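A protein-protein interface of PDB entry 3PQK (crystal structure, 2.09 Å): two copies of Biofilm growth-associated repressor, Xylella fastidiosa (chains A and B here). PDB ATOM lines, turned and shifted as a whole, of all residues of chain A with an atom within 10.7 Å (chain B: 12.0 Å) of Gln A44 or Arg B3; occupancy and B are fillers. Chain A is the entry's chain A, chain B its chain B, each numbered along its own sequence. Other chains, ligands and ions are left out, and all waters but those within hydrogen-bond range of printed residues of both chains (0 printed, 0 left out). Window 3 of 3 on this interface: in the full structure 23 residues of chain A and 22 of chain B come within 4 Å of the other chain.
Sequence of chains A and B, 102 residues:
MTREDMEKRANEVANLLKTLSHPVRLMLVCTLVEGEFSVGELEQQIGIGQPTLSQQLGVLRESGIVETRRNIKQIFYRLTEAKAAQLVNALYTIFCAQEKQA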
ATOM      1  N   PRO A  23       6.686 -27.441 -18.666  1.00  0.00           N
ATOM      2  CA  PRO A  23       6.510 -25.969 -18.708  1.00  0.00           C
ATOM      3  C   PRO A  23       7.049 -25.269 -19.951  1.00  0.00           C
ATOM      4  O   PRO A  23       6.398 -24.362 -20.461  1.00  0.00           O
ATOM      5  CB  PRO A  23       7.207 -25.486 -17.423  1.00  0.00           C
ATOM      6  CG  PRO A  23       8.123 -26.627 -17.015  1.00  0.00           C
ATOM      7  CD  PRO A  23       7.343 -27.860 -17.405  1.00  0.00           C
ATOM      8  N   VAL A  24       8.195 -25.713 -20.477  1.00  0.00           N
ATOM      9  CA  VAL A  24       8.795 -25.112 -21.674  1.00  0.00           C
ATOM     10  C   VAL A  24       7.933 -25.421 -22.898  1.00  0.00           C
ATOM     11  O   VAL A  24       7.642 -24.502 -23.678  1.00  0.00           O
ATOM     12  CB  VAL A  24      10.301 -25.475 -21.865  1.00  0.00           C
ATOM     13  CG1 VAL A  24      10.855 -24.898 -23.173  1.00  0.00           C
ATOM     14  CG2 VAL A  24      11.139 -25.012 -20.662  1.00  0.00           C
ATOM     15  N   MET A  27       4.885 -23.062 -22.687  1.00  0.00           N
ATOM     16  CA  MET A  27       5.190 -21.676 -23.074  1.00  0.00           C
ATOM     17  C   MET A  27       5.296 -21.583 -24.606  1.00  0.00           C
ATOM     18  O   MET A  27       4.657 -20.727 -25.219  1.00  0.00           O
ATOM     19  CB  MET A  27       6.467 -21.189 -22.382  1.00  0.00           C
ATOM     20  CG  MET A  27       6.379 -21.226 -20.871  1.00  0.00           C
ATOM     21  SD  MET A  27       7.956 -20.496 -19.994  1.00  0.00           S
ATOM     22  CE  MET A  27       9.173 -21.887 -20.039  1.00  0.00           C
ATOM     23  N   LEU A  28       5.942 -22.592 -25.221  1.00  0.00           N
ATOM     24  CA  LEU A  28       6.101 -22.681 -26.666  1.00  0.00           C
ATOM     25  C   LEU A  28       4.767 -22.752 -27.389  1.00  0.00           C
ATOM     26  O   LEU A  28       4.531 -21.963 -28.275  1.00  0.00           O
ATOM     27  CB  LEU A  28       7.008 -23.881 -27.023  1.00  0.00           C
ATOM     28  CG  LEU A  28       8.498 -23.672 -26.735  1.00  0.00           C
ATOM     29  CD1 LEU A  28       9.260 -24.973 -26.839  1.00  0.00           C
ATOM     30  CD2 LEU A  28       9.107 -22.601 -27.671  1.00  0.00           C
ATOM     31  N   THR A  31       2.735 -19.485 -26.981  1.00  0.00           N
ATOM     32  CA  THR A  31       3.346 -18.416 -27.795  1.00  0.00           C
ATOM     33  C   THR A  31       2.930 -18.569 -29.269  1.00  0.00           C
ATOM     34  O   THR A  31       2.563 -17.575 -29.913  1.00  0.00           O
ATOM     35  CB  THR A  31       4.882 -18.396 -27.636  1.00  0.00           C
ATOM     36  OG1 THR A  31       5.222 -18.340 -26.246  1.00  0.00           O
ATOM     37  CG2 THR A  31       5.541 -17.227 -28.377  1.00  0.00           C
ATOM     38  N   PHE A  37       6.762 -18.217 -35.325  1.00  0.00           N
ATOM     39  CA  PHE A  37       7.960 -17.562 -34.813  1.00  0.00           C
ATOM     40  C   PHE A  37       9.211 -18.332 -35.149  1.00  0.00           C
ATOM     41  O   PHE A  37       9.192 -19.562 -35.201  1.00  0.00           O
ATOM     42  CB  PHE A  37       7.875 -17.340 -33.298  1.00  0.00           C
ATOM     43  CG  PHE A  37       6.754 -16.425 -32.867  1.00  0.00           C
ATOM     44  CD1 PHE A  37       6.882 -15.039 -32.969  1.00  0.00           C
ATOM     45  CD2 PHE A  37       5.543 -16.943 -32.429  1.00  0.00           C
ATOM     46  CE1 PHE A  37       5.830 -14.190 -32.592  1.00  0.00           C
ATOM     47  CE2 PHE A  37       4.497 -16.094 -32.040  1.00  0.00           C
ATOM     48  CZ  PHE A  37       4.650 -14.724 -32.120  1.00  0.00           C
ATOM     49  N   SER A  38      10.321 -17.612 -35.302  1.00  0.00           N
ATOM     50  CA  SER A  38      11.590 -18.238 -35.594  1.00  0.00           C
ATOM     51  C   SER A  38      12.147 -18.679 -34.246  1.00  0.00           C
ATOM     52  O   SER A  38      11.623 -18.266 -33.221  1.00  0.00           O
ATOM     53  CB  SER A  38      12.518 -17.231 -36.281  1.00  0.00           C
ATOM     54  OG  SER A  38      13.131 -16.421 -35.288  1.00  0.00           O
ATOM     55  N   VAL A  39      13.211 -19.479 -34.236  1.00  0.00           N
ATOM     56  CA  VAL A  39      13.850 -19.986 -33.018  1.00  0.00           C
ATOM     57  C   VAL A  39      14.403 -18.845 -32.164  1.00  0.00           C
ATOM     58  O   VAL A  39      14.260 -18.874 -30.944  1.00  0.00           O
ATOM     59  CB  VAL A  39      14.857 -21.141 -33.327  1.00  0.00           C
ATOM     60  CG1 VAL A  39      16.080 -20.663 -34.116  1.00  0.00           C
ATOM     61  CG2 VAL A  39      15.277 -21.895 -32.073  1.00  0.00           C
ATOM     62  N   GLY A  40      14.957 -17.819 -32.815  1.00  0.00           N
ATOM     63  CA  GLY A  40      15.478 -16.630 -32.143  1.00  0.00           C
ATOM     64  C   GLY A  40      14.392 -15.835 -31.454  1.00  0.00           C
ATOM     65  O   GLY A  40      14.575 -15.405 -30.322  1.00  0.00           O
ATOM     66  N   GLU A  41      13.234 -15.668 -32.122  1.00  0.00           N
ATOM     67  CA  GLU A  41      12.068 -14.977 -31.575  1.00  0.00           C
ATOM     68  C   GLU A  41      11.470 -15.744 -30.404  1.00  0.00           C
ATOM     69  O   GLU A  41      11.025 -15.126 -29.423  1.00  0.00           O
ATOM     70  CB  GLU A  41      11.010 -14.802 -32.663  1.00  0.00           C
ATOM     71  CG  GLU A  41      11.518 -13.942 -33.796  1.00  0.00           C
ATOM     72  CD  GLU A  41      10.608 -13.771 -34.985  1.00  0.00           C
ATOM     73  OE1 GLU A  41       9.902 -14.729 -35.365  1.00  0.00           O
ATOM     74  OE2 GLU A  41      10.626 -12.664 -35.565  1.00  0.00           O
ATOM     75  N   LEU A  42      11.446 -17.103 -30.497  1.00  0.00           N
ATOM     76  CA  LEU A  42      10.929 -17.931 -29.409  1.00  0.00           C
ATOM     77  C   LEU A  42      11.818 -17.795 -28.182  1.00  0.00           C
ATOM     78  O   LEU A  42      11.314 -17.614 -27.078  1.00  0.00           O
ATOM     79  CB  LEU A  42      10.756 -19.415 -29.843  1.00  0.00           C
ATOM     80  CG  LEU A  42       9.618 -19.646 -30.838  1.00  0.00           C
ATOM     81  CD1 LEU A  42       9.754 -20.954 -31.546  1.00  0.00           C
ATOM     82  CD2 LEU A  42       8.242 -19.419 -30.214  1.00  0.00           C
ATOM     83  N   GLU A  43      13.134 -17.827 -28.385  1.00  0.00           N
ATOM     84  CA  GLU A  43      14.134 -17.713 -27.316  1.00  0.00           C
ATOM     85  C   GLU A  43      13.984 -16.416 -26.542  1.00  0.00           C
ATOM     86  O   GLU A  43      14.051 -16.436 -25.318  1.00  0.00           O
ATOM     87  CB  GLU A  43      15.554 -17.860 -27.890  1.00  0.00           C
ATOM     88  CG  GLU A  43      16.682 -17.529 -26.920  1.00  0.00           C
ATOM     89  CD  GLU A  43      18.075 -17.654 -27.502  1.00  0.00           C
ATOM     90  OE1 GLU A  43      18.700 -18.721 -27.313  1.00  0.00           O
ATOM     91  OE2 GLU A  43      18.532 -16.697 -28.166  1.00  0.00           O
ATOM     92  N   GLN A  44      13.782 -15.296 -27.251  1.00  0.00           N
ATOM     93  CA  GLN A  44      13.629 -13.972 -26.645  1.00  0.00           C
ATOM     94  C   GLN A  44      12.331 -13.815 -25.887  1.00  0.00           C
ATOM     95  O   GLN A  44      12.352 -13.323 -24.762  1.00  0.00           O
ATOM     96  CB  GLN A  44      13.783 -12.853 -27.695  1.00  0.00           C
ATOM     97  CG  GLN A  44      15.180 -12.774 -28.322  1.00  0.00           C
ATOM     98  CD  GLN A  44      16.268 -12.500 -27.313  1.00  0.00           C
ATOM     99  OE1 GLN A  44      16.271 -11.466 -26.633  1.00  0.00           O
ATOM    100  NE2 GLN A  44      17.197 -13.438 -27.183  1.00  0.00           N
ATOM    101  N   GLN A  45      11.204 -14.223 -26.489  1.00  0.00           N
ATOM    102  CA  GLN A  45       9.872 -14.122 -25.881  1.00  0.00           C
ATOM    103  C   GLN A  45       9.641 -15.011 -24.622  1.00  0.00           C
ATOM    104  O   GLN A  45       8.866 -14.626 -23.752  1.00  0.00           O
ATOM    105  CB  GLN A  45       8.792 -14.394 -26.929  1.00  0.00           C
ATOM    106  CG  GLN A  45       7.454 -13.723 -26.613  1.00  0.00           C
ATOM    107  CD  GLN A  45       6.461 -13.790 -27.755  1.00  0.00           C
ATOM    108  OE1 GLN A  45       6.816 -13.750 -28.940  1.00  0.00           O
ATOM    109  NE2 GLN A  45       5.181 -13.854 -27.420  1.00  0.00           N
ATOM    110  N   ILE A  46      10.258 -16.193 -24.543  1.00  0.00           N
ATOM    111  CA  ILE A  46      10.010 -17.081 -23.404  1.00  0.00           C
ATOM    112  C   ILE A  46      11.177 -17.115 -22.416  1.00  0.00           C
ATOM    113  O   ILE A  46      10.980 -17.479 -21.258  1.00  0.00           O
ATOM    114  CB  ILE A  46       9.454 -18.496 -23.787  1.00  0.00           C
ATOM    115  CG1 ILE A  46      10.586 -19.478 -24.182  1.00  0.00           C
ATOM    116  CG2 ILE A  46       8.349 -18.414 -24.853  1.00  0.00           C
ATOM    117  CD1 ILE A  46      10.151 -20.969 -24.434  1.00  0.00           C
ATOM    118  N   GLY A  47      12.363 -16.729 -22.868  1.00  0.00           N
ATOM    119  CA  GLY A  47      13.532 -16.694 -22.001  1.00  0.00           C
ATOM    120  C   GLY A  47      14.162 -18.045 -21.762  1.00  0.00           C
ATOM    121  O   GLY A  47      14.685 -18.298 -20.674  1.00  0.00           O
ATOM    122  N   ILE A  48      14.110 -18.921 -22.772  1.00  0.00           N
ATOM    123  CA  ILE A  48      14.708 -20.247 -22.739  1.00  0.00           C
ATOM    124  C   ILE A  48      15.691 -20.318 -23.922  1.00  0.00           C
ATOM    125  O   ILE A  48      15.298 -20.053 -25.064  1.00  0.00           O
ATOM    126  CB  ILE A  48      13.612 -21.368 -22.793  1.00  0.00           C
ATOM    127  CG1 ILE A  48      12.646 -21.330 -21.558  1.00  0.00           C
ATOM    128  CG2 ILE A  48      14.209 -22.769 -23.030  1.00  0.00           C
ATOM    129  CD1 ILE A  48      13.213 -21.836 -20.163  1.00  0.00           C
ATOM    130  N   GLY A  49      16.943 -20.660 -23.636  1.00  0.00           N
ATOM    131  CA  GLY A  49      17.984 -20.752 -24.651  1.00  0.00           C
ATOM    132  C   GLY A  49      18.197 -22.159 -25.162  1.00  0.00           C
ATOM    133  O   GLY A  49      17.271 -22.970 -25.141  1.00  0.00           O
ATOM    134  N   GLN A  50      19.429 -22.454 -25.611  1.00  0.00           N
ATOM    135  CA  GLN A  50      19.837 -23.763 -26.127  1.00  0.00           C
ATOM    136  C   GLN A  50      20.604 -24.586 -25.074  1.00  0.00           C
ATOM    137  O   GLN A  50      21.184 -23.983 -24.179  1.00  0.00           O
ATOM    138  CB  GLN A  50      20.682 -23.613 -27.405  1.00  0.00           C
ATOM    139  CG  GLN A  50      19.912 -23.069 -28.608  1.00  0.00           C
ATOM    140  CD  GLN A  50      18.740 -23.921 -29.033  1.00  0.00           C
ATOM    141  OE1 GLN A  50      18.717 -25.146 -28.846  1.00  0.00           O
ATOM    142  NE2 GLN A  50      17.755 -23.285 -29.653  1.00  0.00           N
ATOM    143  N   LEU A  53      15.509 -25.087 -25.710  1.00  0.00           N
ATOM    144  CA  LEU A  53      14.516 -24.600 -26.679  1.00  0.00           C
ATOM    145  C   LEU A  53      14.360 -25.478 -27.910  1.00  0.00           C
ATOM    146  O   LEU A  53      13.230 -25.809 -28.280  1.00  0.00           O
ATOM    147  CB  LEU A  53      14.789 -23.127 -27.060  1.00  0.00           C
ATOM    148  CG  LEU A  53      13.775 -22.415 -27.961  1.00  0.00           C
ATOM    149  CD1 LEU A  53      12.654 -21.815 -27.159  1.00  0.00           C
ATOM    150  CD2 LEU A  53      14.440 -21.305 -28.697  1.00  0.00           C
ATOM    151  N   LEU A  57      11.171 -28.130 -28.863  1.00  0.00           N
ATOM    152  CA  LEU A  57      10.444 -27.934 -30.125  1.00  0.00           C
ATOM    153  C   LEU A  57      10.523 -29.254 -30.909  1.00  0.00           C
ATOM    154  O   LEU A  57       9.576 -29.631 -31.590  1.00  0.00           O
ATOM    155  CB  LEU A  57      11.038 -26.768 -30.967  1.00  0.00           C
ATOM    156  CG  LEU A  57      10.663 -25.325 -30.539  1.00  0.00           C
ATOM    157  CD1 LEU A  57      11.732 -24.300 -30.989  1.00  0.00           C
ATOM    158  CD2 LEU A  57       9.281 -24.923 -31.032  1.00  0.00           C
ATOM    159  N   GLU A  99      -2.297 -13.802 -18.486  1.00  0.00           N
ATOM    160  CA  GLU A  99      -1.035 -13.090 -18.278  1.00  0.00           C
ATOM    161  C   GLU A  99      -0.946 -11.839 -19.180  1.00  0.00           C
ATOM    162  O   GLU A  99      -0.015 -11.038 -19.026  1.00  0.00           O
ATOM    163  CB  GLU A  99       0.164 -14.036 -18.516  1.00  0.00           C
ATOM    164  N   THR B   2       5.605 -10.566 -17.240  1.00  0.00           N
ATOM    165  CA  THR B   2       7.005 -10.931 -17.010  1.00  0.00           C
ATOM    166  C   THR B   2       7.247 -12.419 -17.286  1.00  0.00           C
ATOM    167  O   THR B   2       6.330 -13.230 -17.126  1.00  0.00           O
ATOM    168  CB  THR B   2       7.462 -10.553 -15.588  1.00  0.00           C
ATOM    169  OG1 THR B   2       6.716 -11.298 -14.628  1.00  0.00           O
ATOM    170  CG2 THR B   2       7.342  -9.057 -15.295  1.00  0.00           C
ATOM    171  N   ARG B   3       8.492 -12.775 -17.676  1.00  0.00           N
ATOM    172  CA  ARG B   3       8.897 -14.152 -17.957  1.00  0.00           C
ATOM    173  C   ARG B   3       8.847 -15.031 -16.709  1.00  0.00           C
ATOM    174  O   ARG B   3       8.619 -16.238 -16.825  1.00  0.00           O
ATOM    175  CB  ARG B   3      10.267 -14.207 -18.636  1.00  0.00           C
ATOM    176  CG  ARG B   3      10.178 -13.694 -20.067  1.00  0.00           C
ATOM    177  CD  ARG B   3      11.501 -13.259 -20.622  1.00  0.00           C
ATOM    178  NE  ARG B   3      11.352 -12.751 -21.991  1.00  0.00           N
ATOM    179  CZ  ARG B   3      11.243 -11.464 -22.318  1.00  0.00           C
ATOM    180  NH1 ARG B   3      11.281 -10.526 -21.378  1.00  0.00           N
ATOM    181  NH2 ARG B   3      11.100 -11.106 -23.588  1.00  0.00           N
ATOM    182  N   GLU B   4       9.029 -14.425 -15.520  1.00  0.00           N
ATOM    183  CA  GLU B   4       8.944 -15.122 -14.242  1.00  0.00           C
ATOM    184  C   GLU B   4       7.477 -15.508 -13.978  1.00  0.00           C
ATOM    185  O   GLU B   4       7.213 -16.628 -13.539  1.00  0.00           O
ATOM    186  CB  GLU B   4       9.497 -14.239 -13.114  1.00  0.00           C
ATOM    187  N   ASP B   5       6.525 -14.597 -14.311  1.00  0.00           N
ATOM    188  CA  ASP B   5       5.090 -14.838 -14.169  1.00  0.00           C
ATOM    189  C   ASP B   5       4.574 -15.875 -15.174  1.00  0.00           C
ATOM    190  O   ASP B   5       3.589 -16.569 -14.879  1.00  0.00           O
ATOM    191  CB  ASP B   5       4.277 -13.538 -14.260  1.00  0.00           C
ATOM    192  CG  ASP B   5       4.341 -12.656 -13.025  1.00  0.00           C
ATOM    193  OD1 ASP B   5       4.298 -13.200 -11.896  1.00  0.00           O
ATOM    194  OD2 ASP B   5       4.398 -11.418 -13.186  1.00  0.00           O
ATOM    195  N   MET B   6       5.239 -15.982 -16.351  1.00  0.00           N
ATOM    196  CA  MET B   6       4.908 -16.947 -17.395  1.00  0.00           C
ATOM    197  C   MET B   6       5.452 -18.306 -16.976  1.00  0.00           C
ATOM    198  O   MET B   6       4.798 -19.317 -17.217  1.00  0.00           O
ATOM    199  CB  MET B   6       5.492 -16.522 -18.746  1.00  0.00           C
ATOM    200  N   GLU B   7       6.649 -18.322 -16.333  1.00  0.00           N
ATOM    201  CA  GLU B   7       7.290 -19.528 -15.790  1.00  0.00           C
ATOM    202  C   GLU B   7       6.438 -20.086 -14.635  1.00  0.00           C
ATOM    203  O   GLU B   7       6.317 -21.302 -14.504  1.00  0.00           O
ATOM    204  CB  GLU B   7       8.711 -19.235 -15.293  1.00  0.00           C
ATOM    205  N   LYS B   8       5.819 -19.195 -13.837  1.00  0.00           N
ATOM    206  CA  LYS B   8       4.967 -19.617 -12.731  1.00  0.00           C
ATOM    207  C   LYS B   8       3.712 -20.341 -13.250  1.00  0.00           C
ATOM    208  O   LYS B   8       3.490 -21.483 -12.853  1.00  0.00           O
ATOM    209  CB  LYS B   8       4.609 -18.446 -11.803  1.00  0.00           C
ATOM    210  N   ARG B   9       2.936 -19.708 -14.172  1.00  0.00           N
ATOM    211  CA  ARG B   9       1.727 -20.302 -14.752  1.00  0.00           C
ATOM    212  C   ARG B   9       2.036 -21.616 -15.482  1.00  0.00           C
ATOM    213  O   ARG B   9       1.298 -22.583 -15.322  1.00  0.00           O
ATOM    214  CB  ARG B   9       1.030 -19.318 -15.709  1.00  0.00           C
ATOM    215  CG  ARG B   9      -0.469 -19.599 -15.886  1.00  0.00           C
ATOM    216  CD  ARG B   9      -1.297 -18.685 -14.991  1.00  0.00           C
ATOM    217  NE  ARG B   9      -2.644 -19.193 -14.711  1.00  0.00           N
ATOM    218  CZ  ARG B   9      -2.936 -20.108 -13.785  1.00  0.00           C
ATOM    219  NH1 ARG B   9      -1.970 -20.674 -13.069  1.00  0.00           N
ATOM    220  NH2 ARG B   9      -4.195 -20.484 -13.587  1.00  0.00           N
ATOM    221  N   ALA B  10       3.140 -21.640 -16.260  1.00  0.00           N
ATOM    222  CA  ALA B  10       3.597 -22.793 -17.033  1.00  0.00           C
ATOM    223  C   ALA B  10       3.785 -24.027 -16.163  1.00  0.00           C
ATOM    224  O   ALA B  10       3.248 -25.076 -16.488  1.00  0.00           O
ATOM    225  CB  ALA B  10       4.891 -22.465 -17.753  1.00  0.00           C
ATOM    226  N   ASN B  11       4.518 -23.893 -15.048  1.00  0.00           N
ATOM    227  CA  ASN B  11       4.757 -24.985 -14.119  1.00  0.00           C
ATOM    228  C   ASN B  11       3.460 -25.495 -13.502  1.00  0.00           C
ATOM    229  O   ASN B  11       3.234 -26.701 -13.444  1.00  0.00           O
ATOM    230  CB  ASN B  11       5.737 -24.549 -13.041  1.00  0.00           C
ATOM    231  CG  ASN B  11       7.168 -24.745 -13.461  1.00  0.00           C
ATOM    232  OD1 ASN B  11       7.628 -25.865 -13.676  1.00  0.00           O
ATOM    233  ND2 ASN B  11       7.897 -23.662 -13.606  1.00  0.00           N
ATOM    234  N   GLU B  12       2.603 -24.565 -13.081  1.00  0.00           N
ATOM    235  CA  GLU B  12       1.320 -24.843 -12.463  1.00  0.00           C
ATOM    236  C   GLU B  12       0.427 -25.650 -13.425  1.00  0.00           C
ATOM    237  O   GLU B  12      -0.146 -26.668 -13.027  1.00  0.00           O
ATOM    238  CB  GLU B  12       0.643 -23.525 -12.040  1.00  0.00           C
ATOM    239  CG  GLU B  12       1.247 -22.886 -10.792  1.00  0.00           C
ATOM    240  CD  GLU B  12       0.727 -21.521 -10.368  1.00  0.00           C
ATOM    241  OE1 GLU B  12      -0.246 -21.016 -10.975  1.00  0.00           O
ATOM    242  OE2 GLU B  12       1.294 -20.961  -9.401  1.00  0.00           O
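Of the printed residues of chain B, Pro A23 touches Ala B10 and Asn B11.
Ser A38 touches none of the printed residues of chain B.
Gly A40 touches none of the printed residues of chain B.
No residue of chain B comes within 4 Å of Glu A43.
Gln A44 touches just one residue of chain B: Arg B3 (2.8 Å).
No residue of chain B comes within 4 Å of Ile A46.
No residue of chain B comes within 4 Å of Gly A47.
No residue of chain A comes within 4 Å of Thr B2.
Arg B3 touches just these residues of chain A: Gln A44 and Gln A45.
No residue of chain A comes within 4 Å of Glu B4.
No residue of chain A comes within 4 Å of Met B6.
No residue of chain A comes within 4 Å of Glu B7.
Arg B9 touches none of the printed residues of chain A.
Printed residues of chain A within 4 Å of Ala B10: Pro A23 and Met A27.
The nearest residue of chain A that does not touch Arg B3 is Ile A46 (4.05 Å).
The nearest printed residue of chain B that does not touch Met A27 is Glu B7 (4.4 Å).
Printed residues of chain B that touch a printed residue of chain A: Arg B3, Ala B10 and Asn B11.
Printed residues of chain A that touch a printed residue of chain B: Pro A23, Met A27, Gln A44 and Gln A45.
Hydrophobic or aromatic side chains of chain A that line the printed part of chain B: Pro A23 and Met A27.
Among the printed residues, 5 pairs touch across the chains.
Among the printed residues, no Asp or Glu carboxylate lies within 4 Å of a Lys or Arg side-chain nitrogen of the other chain.
Ala B10 touches Pro A23 (CB to O, 3.6 Å).
Pro A23 touches Asn B11.
CB of Ala B10 touches CG of Met A27 (3.7 Å).
O of Gln A45 touches NE of Arg B3 (3.6 Å).
O of Met A27 lies within hydrogen-bond range of OG1 of Thr A31 (2.7 Å).
O of Glu B7 lies within hydrogen-bond range of ND2 of Asn B11 (3.0 Å).
The backbone carbonyl oxygen (O) of Gln A44 is in hydrogen-bond range of the guanidinium group (NH2) of Arg B3, at 2.8 Å.
No position is printed for both chains.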
